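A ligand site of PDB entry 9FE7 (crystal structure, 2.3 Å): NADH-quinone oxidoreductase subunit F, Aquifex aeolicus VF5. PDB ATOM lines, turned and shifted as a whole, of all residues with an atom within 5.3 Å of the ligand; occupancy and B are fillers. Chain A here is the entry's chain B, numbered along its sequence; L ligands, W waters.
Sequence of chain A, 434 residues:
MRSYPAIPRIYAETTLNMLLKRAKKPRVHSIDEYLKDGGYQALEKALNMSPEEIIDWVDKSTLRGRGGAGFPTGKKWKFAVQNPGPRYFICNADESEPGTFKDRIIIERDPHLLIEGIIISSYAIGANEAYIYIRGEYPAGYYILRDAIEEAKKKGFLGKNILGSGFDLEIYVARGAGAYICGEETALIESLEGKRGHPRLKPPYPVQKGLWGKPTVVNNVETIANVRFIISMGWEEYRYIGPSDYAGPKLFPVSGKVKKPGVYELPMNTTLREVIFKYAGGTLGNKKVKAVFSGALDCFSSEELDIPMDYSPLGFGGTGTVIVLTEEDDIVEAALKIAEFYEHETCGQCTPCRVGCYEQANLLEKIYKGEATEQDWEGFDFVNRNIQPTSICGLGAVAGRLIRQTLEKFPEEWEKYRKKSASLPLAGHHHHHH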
ATOM      1  N   GLY A  65     -27.673  29.824  13.552  1.00  0.00           N
ATOM      2  CA  GLY A  65     -27.396  28.451  13.155  1.00  0.00           C
ATOM      3  C   GLY A  65     -26.204  27.874  13.933  1.00  0.00           C
ATOM      4  O   GLY A  65     -25.221  28.564  14.188  1.00  0.00           O
ATOM      5  N   ARG A  66     -26.331  26.586  14.280  1.00  0.00           N
ATOM      6  CA  ARG A  66     -25.309  25.898  15.052  1.00  0.00           C
ATOM      7  C   ARG A  66     -24.407  25.034  14.168  1.00  0.00           C
ATOM      8  O   ARG A  66     -23.525  24.355  14.693  1.00  0.00           O
ATOM      9  CB  ARG A  66     -25.995  24.997  16.091  1.00  0.00           C
ATOM     10  CG  ARG A  66     -26.797  25.724  17.157  1.00  0.00           C
ATOM     11  CD  ARG A  66     -26.005  26.619  18.082  1.00  0.00           C
ATOM     12  NE  ARG A  66     -26.849  27.175  19.148  1.00  0.00           N
ATOM     13  CZ  ARG A  66     -27.162  28.451  19.352  1.00  0.00           C
ATOM     14  NH1 ARG A  66     -27.647  28.845  20.527  1.00  0.00           N
ATOM     15  NH2 ARG A  66     -26.922  29.360  18.430  1.00  0.00           N
ATOM     16  N   GLY A  67     -24.586  25.102  12.840  1.00  0.00           N
ATOM     17  CA  GLY A  67     -23.939  24.142  11.955  1.00  0.00           C
ATOM     18  C   GLY A  67     -22.534  24.571  11.541  1.00  0.00           C
ATOM     19  O   GLY A  67     -21.792  23.765  10.979  1.00  0.00           O
ATOM     20  N   GLY A  68     -22.218  25.853  11.776  1.00  0.00           N
ATOM     21  CA  GLY A  68     -20.879  26.401  11.647  1.00  0.00           C
ATOM     22  C   GLY A  68     -20.839  27.806  11.052  1.00  0.00           C
ATOM     23  O   GLY A  68     -19.806  28.465  11.167  1.00  0.00           O
ATOM     24  N   ALA A  69     -21.903  28.221  10.350  1.00  0.00           N
ATOM     25  CA  ALA A  69     -21.882  29.438   9.550  1.00  0.00           C
ATOM     26  C   ALA A  69     -22.655  30.556  10.262  1.00  0.00           C
ATOM     27  O   ALA A  69     -22.593  31.714   9.868  1.00  0.00           O
ATOM     28  CB  ALA A  69     -22.450  29.194   8.166  1.00  0.00           C
ATOM     29  N   GLY A  70     -23.396  30.164  11.314  1.00  0.00           N
ATOM     30  CA  GLY A  70     -23.940  31.115  12.278  1.00  0.00           C
ATOM     31  C   GLY A  70     -25.017  32.030  11.690  1.00  0.00           C
ATOM     32  O   GLY A  70     -25.205  33.145  12.199  1.00  0.00           O
ATOM     33  N   PHE A  71     -25.728  31.544  10.652  1.00  0.00           N
ATOM     34  CA  PHE A  71     -26.718  32.366   9.978  1.00  0.00           C
ATOM     35  C   PHE A  71     -27.952  32.468  10.861  1.00  0.00           C
ATOM     36  O   PHE A  71     -28.460  31.460  11.316  1.00  0.00           O
ATOM     37  CB  PHE A  71     -27.117  31.901   8.570  1.00  0.00           C
ATOM     38  CG  PHE A  71     -27.862  32.980   7.788  1.00  0.00           C
ATOM     39  CD1 PHE A  71     -27.166  33.985   7.096  1.00  0.00           C
ATOM     40  CD2 PHE A  71     -29.259  33.037   7.774  1.00  0.00           C
ATOM     41  CE1 PHE A  71     -27.854  34.977   6.389  1.00  0.00           C
ATOM     42  CE2 PHE A  71     -29.936  34.035   7.088  1.00  0.00           C
ATOM     43  CZ  PHE A  71     -29.229  34.991   6.385  1.00  0.00           C
ATOM     44  N   THR A  73     -31.438  32.203  12.353  1.00  0.00           N
ATOM     45  CA  THR A  73     -32.325  31.130  11.922  1.00  0.00           C
ATOM     46  C   THR A  73     -33.652  31.700  11.427  1.00  0.00           C
ATOM     47  O   THR A  73     -34.140  31.315  10.368  1.00  0.00           O
ATOM     48  CB  THR A  73     -32.519  30.141  13.069  1.00  0.00           C
ATOM     49  OG1 THR A  73     -31.212  29.769  13.479  1.00  0.00           O
ATOM     50  CG2 THR A  73     -33.336  28.931  12.643  1.00  0.00           C
ATOM     51  N   LYS A  76     -33.338  33.174   8.031  1.00  0.00           N
ATOM     52  CA  LYS A  76     -33.268  32.117   7.030  1.00  0.00           C
ATOM     53  C   LYS A  76     -34.672  31.679   6.636  1.00  0.00           C
ATOM     54  O   LYS A  76     -34.986  31.508   5.454  1.00  0.00           O
ATOM     55  CB  LYS A  76     -32.509  30.868   7.486  1.00  0.00           C
ATOM     56  CG  LYS A  76     -32.332  29.806   6.410  1.00  0.00           C
ATOM     57  CD  LYS A  76     -31.622  28.538   6.880  1.00  0.00           C
ATOM     58  CE  LYS A  76     -30.243  28.791   7.415  1.00  0.00           C
ATOM     59  NZ  LYS A  76     -29.539  27.531   7.653  1.00  0.00           N
ATOM     60  N   ASN A  92     -30.124  18.651   9.261  1.00  0.00           N
ATOM     61  CA  ASN A  92     -28.790  18.187   8.930  1.00  0.00           C
ATOM     62  C   ASN A  92     -28.233  17.424  10.145  1.00  0.00           C
ATOM     63  O   ASN A  92     -27.866  18.027  11.151  1.00  0.00           O
ATOM     64  CB  ASN A  92     -27.925  19.347   8.465  1.00  0.00           C
ATOM     65  CG  ASN A  92     -26.559  18.945   7.933  1.00  0.00           C
ATOM     66  OD1 ASN A  92     -26.086  17.823   8.156  1.00  0.00           O
ATOM     67  ND2 ASN A  92     -25.906  19.870   7.251  1.00  0.00           N
ATOM     68  N   ASP A  94     -25.542  15.192   9.745  1.00  0.00           N
ATOM     69  CA  ASP A  94     -24.396  14.523   9.131  1.00  0.00           C
ATOM     70  C   ASP A  94     -23.179  14.518  10.057  1.00  0.00           C
ATOM     71  O   ASP A  94     -22.309  13.668   9.901  1.00  0.00           O
ATOM     72  CB  ASP A  94     -24.039  15.110   7.776  1.00  0.00           C
ATOM     73  CG  ASP A  94     -23.323  14.106   6.884  1.00  0.00           C
ATOM     74  OD1 ASP A  94     -23.924  13.068   6.634  1.00  0.00           O
ATOM     75  OD2 ASP A  94     -22.159  14.340   6.514  1.00  0.00           O
ATOM     76  N   GLU A  95     -23.142  15.468  10.996  1.00  0.00           N
ATOM     77  CA  GLU A  95     -22.088  15.615  11.990  1.00  0.00           C
ATOM     78  C   GLU A  95     -20.924  14.641  11.736  1.00  0.00           C
ATOM     79  O   GLU A  95     -20.954  13.488  12.212  1.00  0.00           O
ATOM     80  CB  GLU A  95     -22.732  15.468  13.366  1.00  0.00           C
ATOM     81  CG  GLU A  95     -21.779  15.738  14.514  1.00  0.00           C
ATOM     82  CD  GLU A  95     -22.432  15.677  15.870  1.00  0.00           C
ATOM     83  OE1 GLU A  95     -22.538  16.737  16.498  1.00  0.00           O
ATOM     84  OE2 GLU A  95     -22.824  14.573  16.305  1.00  0.00           O
ATOM     85  N   SER A  96     -19.915  15.120  10.981  1.00  0.00           N
ATOM     86  CA  SER A  96     -18.772  14.283  10.645  1.00  0.00           C
ATOM     87  C   SER A  96     -17.434  15.014  10.826  1.00  0.00           C
ATOM     88  O   SER A  96     -16.394  14.442  10.516  1.00  0.00           O
ATOM     89  CB  SER A  96     -18.896  13.708   9.249  1.00  0.00           C
ATOM     90  OG  SER A  96     -19.978  12.798   9.203  1.00  0.00           O
ATOM     91  N   ASP A 103     -24.455  16.553  18.390  1.00  0.00           N
ATOM     92  CA  ASP A 103     -25.780  16.372  17.827  1.00  0.00           C
ATOM     93  C   ASP A 103     -26.254  14.947  18.083  1.00  0.00           C
ATOM     94  O   ASP A 103     -27.451  14.697  18.199  1.00  0.00           O
ATOM     95  CB  ASP A 103     -25.804  16.622  16.322  1.00  0.00           C
ATOM     96  CG  ASP A 103     -25.459  18.021  15.832  1.00  0.00           C
ATOM     97  OD1 ASP A 103     -25.487  18.998  16.634  1.00  0.00           O
ATOM     98  OD2 ASP A 103     -25.179  18.133  14.620  1.00  0.00           O
ATOM     99  N   TYR A 180     -18.123  13.298   4.368  1.00  0.00           N
ATOM    100  CA  TYR A 180     -18.192  14.508   5.184  1.00  0.00           C
ATOM    101  C   TYR A 180     -18.838  15.669   4.417  1.00  0.00           C
ATOM    102  O   TYR A 180     -19.543  16.477   5.016  1.00  0.00           O
ATOM    103  CB  TYR A 180     -16.794  14.914   5.654  1.00  0.00           C
ATOM    104  CG  TYR A 180     -16.670  16.307   6.271  1.00  0.00           C
ATOM    105  CD1 TYR A 180     -17.280  16.623   7.474  1.00  0.00           C
ATOM    106  CD2 TYR A 180     -15.939  17.311   5.638  1.00  0.00           C
ATOM    107  CE1 TYR A 180     -17.173  17.886   8.028  1.00  0.00           C
ATOM    108  CE2 TYR A 180     -15.826  18.574   6.183  1.00  0.00           C
ATOM    109  CZ  TYR A 180     -16.443  18.870   7.391  1.00  0.00           C
ATOM    110  OH  TYR A 180     -16.342  20.112   7.950  1.00  0.00           O
ATOM    111  N   ILE A 181     -18.586  15.748   3.111  1.00  0.00           N
ATOM    112  CA  ILE A 181     -19.054  16.839   2.273  1.00  0.00           C
ATOM    113  C   ILE A 181     -20.585  16.851   2.213  1.00  0.00           C
ATOM    114  O   ILE A 181     -21.179  17.862   1.848  1.00  0.00           O
ATOM    115  CB  ILE A 181     -18.408  16.788   0.861  1.00  0.00           C
ATOM    116  CG1 ILE A 181     -18.555  18.119   0.109  1.00  0.00           C
ATOM    117  CG2 ILE A 181     -18.925  15.641   0.003  1.00  0.00           C
ATOM    118  CD1 ILE A 181     -17.963  19.312   0.843  1.00  0.00           C
ATOM    119  N   GLY A 183     -22.541  16.976   4.526  1.00  0.00           N
ATOM    120  CA  GLY A 183     -22.996  17.923   5.537  1.00  0.00           C
ATOM    121  C   GLY A 183     -23.108  19.349   5.000  1.00  0.00           C
ATOM    122  O   GLY A 183     -23.842  20.143   5.565  1.00  0.00           O
ATOM    123  N   GLU A 184     -22.358  19.662   3.931  1.00  0.00           N
ATOM    124  CA  GLU A 184     -22.520  20.926   3.222  1.00  0.00           C
ATOM    125  C   GLU A 184     -23.908  20.873   2.585  1.00  0.00           C
ATOM    126  O   GLU A 184     -24.265  19.867   1.982  1.00  0.00           O
ATOM    127  CB  GLU A 184     -21.369  21.169   2.241  1.00  0.00           C
ATOM    128  CG  GLU A 184     -21.314  22.588   1.683  1.00  0.00           C
ATOM    129  CD  GLU A 184     -22.253  22.928   0.524  1.00  0.00           C
ATOM    130  OE1 GLU A 184     -22.819  22.008  -0.086  1.00  0.00           O
ATOM    131  OE2 GLU A 184     -22.419  24.133   0.238  1.00  0.00           O
ATOM    132  N   GLU A 185     -24.713  21.909   2.819  1.00  0.00           N
ATOM    133  CA  GLU A 185     -26.153  21.854   2.582  1.00  0.00           C
ATOM    134  C   GLU A 185     -26.522  21.569   1.120  1.00  0.00           C
ATOM    135  O   GLU A 185     -27.517  20.888   0.883  1.00  0.00           O
ATOM    136  CB  GLU A 185     -26.806  23.150   3.094  1.00  0.00           C
ATOM    137  CG  GLU A 185     -26.210  24.433   2.539  1.00  0.00           C
ATOM    138  CD  GLU A 185     -26.652  25.649   3.338  1.00  0.00           C
ATOM    139  OE1 GLU A 185     -27.877  25.791   3.545  1.00  0.00           O
ATOM    140  OE2 GLU A 185     -25.755  26.445   3.718  1.00  0.00           O
ATOM    141  N   VAL A 218     -32.416  24.317   5.371  1.00  0.00           N
ATOM    142  CA  VAL A 218     -31.572  23.370   6.054  1.00  0.00           C
ATOM    143  C   VAL A 218     -31.178  23.969   7.390  1.00  0.00           C
ATOM    144  O   VAL A 218     -30.724  25.109   7.447  1.00  0.00           O
ATOM    145  CB  VAL A 218     -30.345  22.999   5.204  1.00  0.00           C
ATOM    146  CG1 VAL A 218     -29.453  22.009   5.950  1.00  0.00           C
ATOM    147  CG2 VAL A 218     -30.755  22.465   3.853  1.00  0.00           C
ATOM    148  N   ASN A 219     -31.410  23.206   8.469  1.00  0.00           N
ATOM    149  CA  ASN A 219     -30.993  23.579   9.804  1.00  0.00           C
ATOM    150  C   ASN A 219     -30.297  22.392  10.468  1.00  0.00           C
ATOM    151  O   ASN A 219     -30.595  21.232  10.162  1.00  0.00           O
ATOM    152  CB  ASN A 219     -32.142  24.129  10.655  1.00  0.00           C
ATOM    153  CG  ASN A 219     -32.408  25.587  10.346  1.00  0.00           C
ATOM    154  OD1 ASN A 219     -33.536  25.968   9.996  1.00  0.00           O
ATOM    155  ND2 ASN A 219     -31.367  26.400  10.449  1.00  0.00           N
ATOM    156  N   ASN A 220     -29.344  22.738  11.335  1.00  0.00           N
ATOM    157  CA  ASN A 220     -28.555  21.792  12.102  1.00  0.00           C
ATOM    158  C   ASN A 220     -29.398  21.250  13.237  1.00  0.00           C
ATOM    159  O   ASN A 220     -30.254  21.960  13.747  1.00  0.00           O
ATOM    160  CB  ASN A 220     -27.283  22.449  12.629  1.00  0.00           C
ATOM    161  CG  ASN A 220     -26.518  21.565  13.581  1.00  0.00           C
ATOM    162  OD1 ASN A 220     -25.878  20.588  13.171  1.00  0.00           O
ATOM    163  ND2 ASN A 220     -26.533  21.924  14.857  1.00  0.00           N
ATOM    164  N   VAL A 221     -29.130  19.991  13.632  1.00  0.00           N
ATOM    165  CA  VAL A 221     -29.796  19.302  14.733  1.00  0.00           C
ATOM    166  C   VAL A 221     -29.908  20.202  15.965  1.00  0.00           C
ATOM    167  O   VAL A 221     -31.000  20.397  16.483  1.00  0.00           O
ATOM    168  CB  VAL A 221     -29.034  18.006  15.041  1.00  0.00           C
ATOM    169  CG1 VAL A 221     -29.383  17.443  16.428  1.00  0.00           C
ATOM    170  CG2 VAL A 221     -29.269  16.938  13.969  1.00  0.00           C
ATOM    171  N   THR A 223     -29.584  23.400  16.275  1.00  0.00           N
ATOM    172  CA  THR A 223     -30.380  24.592  15.993  1.00  0.00           C
ATOM    173  C   THR A 223     -31.867  24.276  16.246  1.00  0.00           C
ATOM    174  O   THR A 223     -32.577  25.035  16.895  1.00  0.00           O
ATOM    175  CB  THR A 223     -30.190  25.063  14.549  1.00  0.00           C
ATOM    176  OG1 THR A 223     -28.809  25.265  14.283  1.00  0.00           O
ATOM    177  CG2 THR A 223     -30.964  26.336  14.254  1.00  0.00           C
ATOM    178  N   CYS A 393     -17.204  25.662  -2.292  1.00  0.00           N
ATOM    179  CA  CYS A 393     -17.749  25.516  -0.958  1.00  0.00           C
ATOM    180  C   CYS A 393     -16.654  25.765   0.076  1.00  0.00           C
ATOM    181  O   CYS A 393     -15.474  25.893  -0.272  1.00  0.00           O
ATOM    182  CB  CYS A 393     -18.443  24.160  -0.791  1.00  0.00           C
ATOM    183  SG  CYS A 393     -17.343  22.806  -0.314  1.00  0.00           S
ATOM    184  N   GLY A 394     -17.053  25.792   1.358  1.00  0.00           N
ATOM    185  CA  GLY A 394     -16.181  26.218   2.447  1.00  0.00           C
ATOM    186  C   GLY A 394     -15.051  25.236   2.749  1.00  0.00           C
ATOM    187  O   GLY A 394     -14.099  25.602   3.437  1.00  0.00           O
ATOM    188  N   LEU A 395     -15.132  23.993   2.251  1.00  0.00           N
ATOM    189  CA  LEU A 395     -14.144  22.982   2.599  1.00  0.00           C
ATOM    190  C   LEU A 395     -12.778  23.433   2.065  1.00  0.00           C
ATOM    191  O   LEU A 395     -11.770  23.336   2.769  1.00  0.00           O
ATOM    192  CB  LEU A 395     -14.508  21.597   2.077  1.00  0.00           C
ATOM    193  CG  LEU A 395     -13.594  20.449   2.541  1.00  0.00           C
ATOM    194  CD1 LEU A 395     -14.328  19.116   2.588  1.00  0.00           C
ATOM    195  CD2 LEU A 395     -12.373  20.321   1.633  1.00  0.00           C
HETATM  196  N1  LIG L   1     -23.877  21.740   9.008  1.00  0.00           N
HETATM  197  C1  LIG L   1     -24.421  20.789   9.869  1.00  0.00           C
HETATM  198  O1  LIG L   1     -25.455  20.998  10.524  1.00  0.00           O
HETATM  199  N2  LIG L   1     -23.833  19.564   9.998  1.00  0.00           N
HETATM  200  C2  LIG L   1     -22.706  19.138   9.329  1.00  0.00           C
HETATM  201  O2  LIG L   1     -22.248  18.033   9.579  1.00  0.00           O
HETATM  202  C3  LIG L   1     -22.140  20.119   8.403  1.00  0.00           C
HETATM  203  N3  LIG L   1     -21.107  19.767   7.692  1.00  0.00           N
HETATM  204  C4  LIG L   1     -20.593  20.695   6.797  1.00  0.00           C
HETATM  205  C5  LIG L   1     -19.504  20.321   6.013  1.00  0.00           C
HETATM  206  C6  LIG L   1     -18.918  21.213   5.126  1.00  0.00           C
HETATM  207  C7  LIG L   1     -17.689  20.798   4.357  1.00  0.00           C
HETATM  208  C8  LIG L   1     -19.455  22.507   4.991  1.00  0.00           C
HETATM  209  C9  LIG L   1     -18.814  23.523   4.071  1.00  0.00           C
HETATM  210  C10 LIG L   1     -20.564  22.867   5.748  1.00  0.00           C
HETATM  211  C11 LIG L   1     -21.131  21.979   6.661  1.00  0.00           C
HETATM  212  N4  LIG L   1     -22.268  22.324   7.458  1.00  0.00           N
HETATM  213  C12 LIG L   1     -22.788  21.400   8.325  1.00  0.00           C
HETATM  214  C13 LIG L   1     -22.930  23.621   7.349  1.00  0.00           C
HETATM  215  C14 LIG L   1     -24.161  23.558   6.465  1.00  0.00           C
HETATM  216  O3  LIG L   1     -23.801  23.693   5.080  1.00  0.00           O
HETATM  217  C15 LIG L   1     -25.178  24.643   6.855  1.00  0.00           C
HETATM  218  O4  LIG L   1     -24.493  25.843   7.204  1.00  0.00           O
HETATM  219  C16 LIG L   1     -26.045  24.285   8.057  1.00  0.00           C
HETATM  220  O5  LIG L   1     -26.396  22.908   8.039  1.00  0.00           O
HETATM  221  C17 LIG L   1     -27.261  25.177   8.146  1.00  0.00           C
HETATM  222  O6  LIG L   1     -27.909  24.937   9.411  1.00  0.00           O
HETATM  223  P1  LIG L   1     -27.725  25.980  10.592  1.00  0.00           P
HETATM  224  O7  LIG L   1     -26.391  25.879  11.198  1.00  0.00           O
HETATM  225  O8  LIG L   1     -28.079  27.319  10.053  1.00  0.00           O
HETATM  226  O9  LIG L   1     -28.860  25.565  11.561  1.00  0.00           O
HETATM  227  O   HOH W   1     -20.836  16.216   7.636  1.00  0.00           O
HETATM  228  O   HOH W   2     -25.902  29.105   9.558  1.00  0.00           O
HETATM  229  O   HOH W   3     -24.268  26.672   9.724  1.00  0.00           O
HETATM  230  O   HOH W   4     -19.802  17.963  10.817  1.00  0.00           O
HETATM  231  O   HOH W   5     -18.976  24.232   8.453  1.00  0.00           O
HETATM  232  O   HOH W   6     -20.507  21.497  10.705  1.00  0.00           O
HETATM  233  O   HOH W   7     -29.899  29.175  11.055  1.00  0.00           O
HETATM  234  O   HOH W   8     -25.270  17.492  11.827  1.00  0.00           O
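The side-chain amide nitrogen (ND2) of Asn 92 sits close to an oxygen (O5) of the ligand (3.2 Å).
N of Arg 66 is in hydrogen-bond range of O7 of the ligand (3.2 Å).
O3 of the ligand sits at hydrogen-bond distance from N of Glu 185 (3.0 Å).
The side-chain amide oxygen (OD1) of Asn 220 sits close to an oxygen (O1) of the ligand, at 2.7 Å.
N of Gly 67 sits at hydrogen-bond distance from O7 of the ligand, 2.6 Å away.
N of Glu 95 is in hydrogen-bond range of O2 of the ligand, at 3.1 Å.
The side-chain amino group (NZ) of Lys 76 is in salt-bridge range of an oxygen (O8) of the ligand, 2.8 Å away.
The side-chain amide nitrogen (ND2) of Asn 219 is in hydrogen-bond range of an oxygen (O9) of the ligand, 2.9 Å away.
N of Asn 220 is in hydrogen-bond range of O9 of the ligand (2.9 Å).
The side-chain hydroxyl (OG1) of Thr 223 is in hydrogen-bond range of an oxygen (O9) of the ligand (2.7 Å).
The backbone carbonyl oxygen (O) of Val 218 lies within hydrogen-bond range of the side-chain amino group (NZ) of Lys 76.
The backbone NH (N) of Asp 103 sits at hydrogen-bond distance from the side-chain carboxylate (OE1) of Glu 95 (2.7 Å).
ND2 of Asn 92 is in hydrogen-bond range of O of Gly 183, at 2.7 Å.
The side-chain hydroxyl of Thr 223 is in hydrogen-bond range of the backbone NH of Arg 66 (2.8 Å).
SG of Cys 393 lies close to N of Leu 395 (3.6 Å).
The backbone NH (N) of Asn 92 lies within hydrogen-bond range of the backbone carbonyl oxygen (O) of Asn 219.
The backbone NH of Val 221 lies close to the backbone carbonyl oxygen of Asn 92.
OD1 of Asn 220 sits close to OD2 of Asp 103.
The backbone carbonyl oxygen (O) of Gly 183 lies close to a nitrogen (N4) of the ligand.
The backbone carbonyl oxygen of Val 218 lies close to an oxygen (O6) of the ligand, 3.4 Å away.
Gly 65 touches the ligand.
C of Asp 94 touches O2 of the ligand, at 3.7 Å.
Ser 96 touches the ligand.
Tyr 180 touches the ligand.
CD1 of Ile 181 touches C7 of the ligand, at 3.8 Å.
N of Glu 184 touches C4 of the ligand, 3.5 Å away.
N of Gly 394 touches C9 of the ligand (3.95 Å).
CB of Leu 395 touches C7 of the ligand, at 3.99 Å.
Hydrophobic or aromatic side chains within 4 Å of the ligand: Tyr 180, Ile 181, Val 218 and Leu 395.
19 residues have an atom within 4 Å of the ligand: Gly 65, Arg 66, Gly 67, Lys 76, Asn 92, Asp 94, Glu 95, Ser 96, Tyr 180, Ile 181, Gly 183, Glu 184, Glu 185, Val 218, Asn 219, Asn 220, Thr 223, Gly 394 and Leu 395.
Water W3 lies within hydrogen-bond range of an oxygen (O4) of the ligand, the backbone NH of Ala 69 and the backbone NH of Gly 68.
Water W4 bridges an oxygen (O2) of the ligand (2.7 Å) and the backbone NH of Ser 96 (2.8 Å).
Water W7 lies within hydrogen-bond range of the backbone carbonyl oxygen of Phe 71 (2.7 Å), an oxygen (O8) of the ligand (2.8 Å), the side-chain hydroxyl of Thr 73 (2.8 Å), the side-chain amide nitrogen of Asn 219 (3.2 Å) and the backbone NH of Gly 65 (3.4 Å).
Water W2 lies within hydrogen-bond range of N of Phe 71 (2.7 Å), O8 of the ligand (2.9 Å) and N of Gly 70 (3.2 Å).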
